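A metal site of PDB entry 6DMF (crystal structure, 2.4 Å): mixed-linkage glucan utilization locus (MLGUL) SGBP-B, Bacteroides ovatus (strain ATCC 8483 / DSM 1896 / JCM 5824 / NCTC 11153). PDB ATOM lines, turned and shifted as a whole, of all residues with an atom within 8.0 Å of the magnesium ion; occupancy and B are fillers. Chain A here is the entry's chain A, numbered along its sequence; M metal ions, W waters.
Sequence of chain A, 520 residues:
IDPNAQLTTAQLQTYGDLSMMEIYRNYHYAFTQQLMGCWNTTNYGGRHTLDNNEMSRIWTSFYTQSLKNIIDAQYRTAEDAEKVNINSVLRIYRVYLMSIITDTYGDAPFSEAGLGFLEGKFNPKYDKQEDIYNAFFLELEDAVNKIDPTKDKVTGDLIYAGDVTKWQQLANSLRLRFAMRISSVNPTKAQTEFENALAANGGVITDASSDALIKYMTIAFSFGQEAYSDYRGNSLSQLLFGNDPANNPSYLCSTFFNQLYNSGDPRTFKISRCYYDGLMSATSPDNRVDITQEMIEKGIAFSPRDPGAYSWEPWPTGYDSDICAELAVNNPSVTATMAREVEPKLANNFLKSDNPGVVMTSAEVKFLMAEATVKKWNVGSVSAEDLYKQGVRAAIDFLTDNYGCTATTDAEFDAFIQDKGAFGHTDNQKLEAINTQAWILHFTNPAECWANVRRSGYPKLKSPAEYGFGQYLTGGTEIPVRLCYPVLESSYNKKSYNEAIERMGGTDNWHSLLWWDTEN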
ATOM      1  N   TRP A 450      -5.653  29.902  -8.266  1.00  0.00           N
ATOM      2  CA  TRP A 450      -6.828  29.785  -7.365  1.00  0.00           C
ATOM      3  C   TRP A 450      -6.602  28.676  -6.315  1.00  0.00           C
ATOM      4  O   TRP A 450      -6.892  28.877  -5.128  1.00  0.00           O
ATOM      5  CB  TRP A 450      -8.137  29.591  -8.148  1.00  0.00           C
ATOM      6  CG  TRP A 450      -9.371  29.670  -7.289  1.00  0.00           C
ATOM      7  CD1 TRP A 450      -9.547  30.443  -6.177  1.00  0.00           C
ATOM      8  CD2 TRP A 450     -10.612  28.965  -7.483  1.00  0.00           C
ATOM      9  NE1 TRP A 450     -10.789  30.245  -5.651  1.00  0.00           N
ATOM     10  CE2 TRP A 450     -11.464  29.349  -6.431  1.00  0.00           C
ATOM     11  CE3 TRP A 450     -11.066  28.039  -8.425  1.00  0.00           C
ATOM     12  CZ2 TRP A 450     -12.763  28.837  -6.316  1.00  0.00           C
ATOM     13  CZ3 TRP A 450     -12.343  27.526  -8.298  1.00  0.00           C
ATOM     14  CH2 TRP A 450     -13.180  27.934  -7.256  1.00  0.00           C
ATOM     15  N   ALA A 451      -6.062  27.532  -6.748  1.00  0.00           N
ATOM     16  CA  ALA A 451      -5.747  26.431  -5.829  1.00  0.00           C
ATOM     17  C   ALA A 451      -4.813  26.903  -4.707  1.00  0.00           C
ATOM     18  O   ALA A 451      -5.060  26.622  -3.531  1.00  0.00           O
ATOM     19  CB  ALA A 451      -5.135  25.271  -6.577  1.00  0.00           C
ATOM     20  N   ASN A 452      -3.735  27.610  -5.072  1.00  0.00           N
ATOM     21  CA  ASN A 452      -2.702  27.926  -4.090  1.00  0.00           C
ATOM     22  C   ASN A 452      -3.189  29.031  -3.142  1.00  0.00           C
ATOM     23  O   ASN A 452      -2.797  29.059  -1.973  1.00  0.00           O
ATOM     24  CB  ASN A 452      -1.366  28.310  -4.729  1.00  0.00           C
ATOM     25  CG  ASN A 452      -0.275  28.375  -3.690  1.00  0.00           C
ATOM     26  OD1 ASN A 452       0.109  27.351  -3.126  1.00  0.00           O
ATOM     27  ND2 ASN A 452       0.164  29.581  -3.359  1.00  0.00           N
ATOM     28  N   VAL A 453      -4.032  29.935  -3.652  1.00  0.00           N
ATOM     29  CA  VAL A 453      -4.674  30.977  -2.821  1.00  0.00           C
ATOM     30  C   VAL A 453      -5.544  30.294  -1.757  1.00  0.00           C
ATOM     31  O   VAL A 453      -5.469  30.632  -0.582  1.00  0.00           O
ATOM     32  CB  VAL A 453      -5.491  31.983  -3.661  1.00  0.00           C
ATOM     33  CG1 VAL A 453      -6.412  32.850  -2.803  1.00  0.00           C
ATOM     34  CG2 VAL A 453      -4.591  32.875  -4.497  1.00  0.00           C
ATOM     35  N   ARG A 454      -6.359  29.329  -2.178  1.00  0.00           N
ATOM     36  CA  ARG A 454      -7.282  28.639  -1.267  1.00  0.00           C
ATOM     37  C   ARG A 454      -6.501  27.841  -0.222  1.00  0.00           C
ATOM     38  O   ARG A 454      -6.896  27.796   0.955  1.00  0.00           O
ATOM     39  CB  ARG A 454      -8.233  27.716  -2.031  1.00  0.00           C
ATOM     40  CG  ARG A 454      -9.380  28.453  -2.726  1.00  0.00           C
ATOM     41  CD  ARG A 454     -10.181  27.531  -3.624  1.00  0.00           C
ATOM     42  NE  ARG A 454      -9.415  27.107  -4.790  1.00  0.00           N
ATOM     43  CZ  ARG A 454      -9.809  26.173  -5.644  1.00  0.00           C
ATOM     44  NH1 ARG A 454     -10.951  25.536  -5.436  1.00  0.00           N
ATOM     45  NH2 ARG A 454      -9.067  25.887  -6.701  1.00  0.00           N
ATOM     46  N   ARG A 455      -5.394  27.218  -0.661  1.00  0.00           N
ATOM     47  CA  ARG A 455      -4.635  26.273   0.166  1.00  0.00           C
ATOM     48  C   ARG A 455      -3.824  27.032   1.226  1.00  0.00           C
ATOM     49  O   ARG A 455      -3.938  26.730   2.427  1.00  0.00           O
ATOM     50  CB  ARG A 455      -3.729  25.396  -0.709  1.00  0.00           C
ATOM     51  CG  ARG A 455      -2.958  24.330   0.053  1.00  0.00           C
ATOM     52  CD  ARG A 455      -1.691  24.800   0.768  1.00  0.00           C
ATOM     53  NE  ARG A 455      -0.717  25.434  -0.116  1.00  0.00           N
ATOM     54  CZ  ARG A 455       0.451  25.949   0.293  1.00  0.00           C
ATOM     55  NH1 ARG A 455       0.829  25.835   1.556  1.00  0.00           N
ATOM     56  NH2 ARG A 455       1.235  26.562  -0.571  1.00  0.00           N
ATOM     57  N   SER A 456      -3.006  27.992   0.768  1.00  0.00           N
ATOM     58  CA  SER A 456      -2.060  28.720   1.631  1.00  0.00           C
ATOM     59  C   SER A 456      -2.780  29.762   2.507  1.00  0.00           C
ATOM     60  O   SER A 456      -2.342  30.042   3.621  1.00  0.00           O
ATOM     61  CB  SER A 456      -0.971  29.365   0.812  1.00  0.00           C
ATOM     62  OG  SER A 456      -1.471  30.419   0.001  1.00  0.00           O
ATOM     63  N   GLY A 457      -3.883  30.330   2.006  1.00  0.00           N
ATOM     64  CA  GLY A 457      -4.653  31.384   2.694  1.00  0.00           C
ATOM     65  C   GLY A 457      -4.092  32.783   2.449  1.00  0.00           C
ATOM     66  O   GLY A 457      -4.466  33.722   3.137  1.00  0.00           O
ATOM     67  N   TYR A 458      -3.197  32.909   1.459  1.00  0.00           N
ATOM     68  CA  TYR A 458      -2.507  34.172   1.107  1.00  0.00           C
ATOM     69  C   TYR A 458      -2.613  34.411  -0.393  1.00  0.00           C
ATOM     70  O   TYR A 458      -2.606  33.461  -1.171  1.00  0.00           O
ATOM     71  CB  TYR A 458      -1.031  34.138   1.516  1.00  0.00           C
ATOM     72  CG  TYR A 458      -0.766  34.131   2.996  1.00  0.00           C
ATOM     73  CD1 TYR A 458      -0.978  35.258   3.765  1.00  0.00           C
ATOM     74  CD2 TYR A 458      -0.279  32.992   3.623  1.00  0.00           C
ATOM     75  CE1 TYR A 458      -0.738  35.251   5.130  1.00  0.00           C
ATOM     76  CE2 TYR A 458      -0.031  32.974   4.982  1.00  0.00           C
ATOM     77  CZ  TYR A 458      -0.253  34.108   5.744  1.00  0.00           C
ATOM     78  OH  TYR A 458      -0.011  34.077   7.085  1.00  0.00           O
ATOM     79  N   VAL A 481     -15.297  28.595  -2.814  1.00  0.00           N
ATOM     80  CA  VAL A 481     -14.062  27.841  -2.548  1.00  0.00           C
ATOM     81  C   VAL A 481     -14.009  26.600  -3.450  1.00  0.00           C
ATOM     82  O   VAL A 481     -13.052  25.838  -3.397  1.00  0.00           O
ATOM     83  CB  VAL A 481     -13.954  27.453  -1.062  1.00  0.00           C
ATOM     84  CG1 VAL A 481     -13.653  28.669  -0.192  1.00  0.00           C
ATOM     85  CG2 VAL A 481     -15.204  26.741  -0.565  1.00  0.00           C
ATOM     86  N   LEU A 513     -15.800  23.533   1.554  1.00  0.00           N
ATOM     87  CA  LEU A 513     -14.348  23.406   1.457  1.00  0.00           C
ATOM     88  C   LEU A 513     -13.987  22.048   0.849  1.00  0.00           C
ATOM     89  O   LEU A 513     -14.498  21.006   1.277  1.00  0.00           O
ATOM     90  CB  LEU A 513     -13.719  23.567   2.850  1.00  0.00           C
ATOM     91  CG  LEU A 513     -13.812  24.962   3.448  1.00  0.00           C
ATOM     92  CD1 LEU A 513     -13.392  24.962   4.910  1.00  0.00           C
ATOM     93  CD2 LEU A 513     -12.965  25.954   2.655  1.00  0.00           C
ATOM     94  N   LEU A 514     -13.110  22.073  -0.163  1.00  0.00           N
ATOM     95  CA  LEU A 514     -12.481  20.881  -0.712  1.00  0.00           C
ATOM     96  C   LEU A 514     -11.660  20.210   0.402  1.00  0.00           C
ATOM     97  O   LEU A 514     -11.254  20.903   1.342  1.00  0.00           O
ATOM     98  CB  LEU A 514     -11.574  21.266  -1.880  1.00  0.00           C
ATOM     99  CG  LEU A 514     -12.280  21.901  -3.080  1.00  0.00           C
ATOM    100  CD1 LEU A 514     -11.265  22.393  -4.097  1.00  0.00           C
ATOM    101  CD2 LEU A 514     -13.230  20.919  -3.717  1.00  0.00           C
ATOM    102  N   TRP A 516      -8.585  19.250   0.681  1.00  0.00           N
ATOM    103  CA  TRP A 516      -7.238  19.824   0.987  1.00  0.00           C
ATOM    104  C   TRP A 516      -7.319  21.259   1.528  1.00  0.00           C
ATOM    105  O   TRP A 516      -6.296  21.787   1.998  1.00  0.00           O
ATOM    106  CB  TRP A 516      -6.275  19.743  -0.206  1.00  0.00           C
ATOM    107  CG  TRP A 516      -6.719  20.318  -1.515  1.00  0.00           C
ATOM    108  CD1 TRP A 516      -6.957  19.604  -2.646  1.00  0.00           C
ATOM    109  CD2 TRP A 516      -6.885  21.702  -1.892  1.00  0.00           C
ATOM    110  NE1 TRP A 516      -7.283  20.429  -3.681  1.00  0.00           N
ATOM    111  CE2 TRP A 516      -7.246  21.721  -3.251  1.00  0.00           C
ATOM    112  CE3 TRP A 516      -6.772  22.928  -1.212  1.00  0.00           C
ATOM    113  CZ2 TRP A 516      -7.511  22.907  -3.942  1.00  0.00           C
ATOM    114  CZ3 TRP A 516      -7.030  24.098  -1.900  1.00  0.00           C
ATOM    115  CH2 TRP A 516      -7.388  24.084  -3.244  1.00  0.00           C
ATOM    116  N   ASP A 517      -8.489  21.886   1.455  1.00  0.00           N
ATOM    117  CA  ASP A 517      -8.707  23.261   1.927  1.00  0.00           C
ATOM    118  C   ASP A 517      -9.288  23.185   3.335  1.00  0.00           C
ATOM    119  O   ASP A 517     -10.449  22.821   3.510  1.00  0.00           O
ATOM    120  CB  ASP A 517      -9.583  24.027   0.932  1.00  0.00           C
ATOM    121  CG  ASP A 517      -9.570  25.549   1.043  1.00  0.00           C
ATOM    122  OD1 ASP A 517      -8.861  26.070   1.927  1.00  0.00           O
ATOM    123  OD2 ASP A 517     -10.277  26.194   0.235  1.00  0.00           O
ATOM    124  N   THR A 518      -8.459  23.501   4.349  1.00  0.00           N
ATOM    125  CA  THR A 518      -8.842  23.347   5.762  1.00  0.00           C
ATOM    126  C   THR A 518      -9.489  24.626   6.313  1.00  0.00           C
ATOM    127  O   THR A 518     -10.335  24.541   7.201  1.00  0.00           O
ATOM    128  CB  THR A 518      -7.630  22.951   6.621  1.00  0.00           C
ATOM    129  OG1 THR A 518      -6.701  24.044   6.612  1.00  0.00           O
ATOM    130  CG2 THR A 518      -6.947  21.698   6.131  1.00  0.00           C
ATOM    131  N   GLU A 519      -9.082  25.794   5.803  1.00  0.00           N
ATOM    132  CA  GLU A 519      -9.557  27.100   6.269  1.00  0.00           C
ATOM    133  C   GLU A 519     -10.093  27.913   5.076  1.00  0.00           C
ATOM    134  O   GLU A 519      -9.629  27.754   3.948  1.00  0.00           O
ATOM    135  CB  GLU A 519      -8.431  27.912   6.918  1.00  0.00           C
ATOM    136  CG  GLU A 519      -8.013  27.407   8.287  1.00  0.00           C
ATOM    137  CD  GLU A 519      -6.929  28.252   8.943  1.00  0.00           C
ATOM    138  OE1 GLU A 519      -6.669  29.369   8.438  1.00  0.00           O
ATOM    139  OE2 GLU A 519      -6.350  27.788   9.950  1.00  0.00           O
ATOM    140  N   ASN A 520     -11.020  28.830   5.370  1.00  0.00           N
ATOM    141  CA  ASN A 520     -11.706  29.618   4.355  1.00  0.00           C
ATOM    142  C   ASN A 520     -10.829  30.815   3.970  1.00  0.00           C
ATOM    143  O   ASN A 520     -10.791  31.820   4.664  1.00  0.00           O
ATOM    144  CB  ASN A 520     -13.105  30.051   4.835  1.00  0.00           C
ATOM    145  CG  ASN A 520     -14.120  29.950   3.731  1.00  0.00           C
ATOM    146  OD1 ASN A 520     -13.911  30.493   2.640  1.00  0.00           O
ATOM    147  ND2 ASN A 520     -15.206  29.229   3.975  1.00  0.00           N
HETATM  148 MG    MG M   1      -8.550  28.340   2.334  1.00  0.00          MG
HETATM  149  O   HOH W   1     -10.002  28.876   0.604  1.00  0.00           O
HETATM  150  O   HOH W   2      -7.696  29.918   2.998  1.00  0.00           O
HETATM  151  O   HOH W   3      -6.929  27.364   3.645  1.00  0.00           O
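The magnesium ion is bound by water W2 (1.9 Å), O of Glu 519 (2.0 Å), O of Arg 454 (2.2 Å), water W3 (2.3 Å), water W1 (2.3 Å) and OD1 of Asp 517 (2.3 Å).
The guanidinium group (NE) of Arg 454 sits at hydrogen-bond distance from the backbone carbonyl oxygen (O) of Trp 450, at 3.1 Å. O of Val 481 sits at hydrogen-bond distance from NH1 of Arg 454 (2.9 Å).
Water W3 bridges the backbone carbonyl oxygen of Arg 455 (3.3 Å) and the backbone NH of Glu 519 (3.4 Å).
Residues that only touch the magnesium ion: Asn 520 (3.7 Å). Of the 17 residues printed, 4 come within 4 Å of the magnesium ion.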
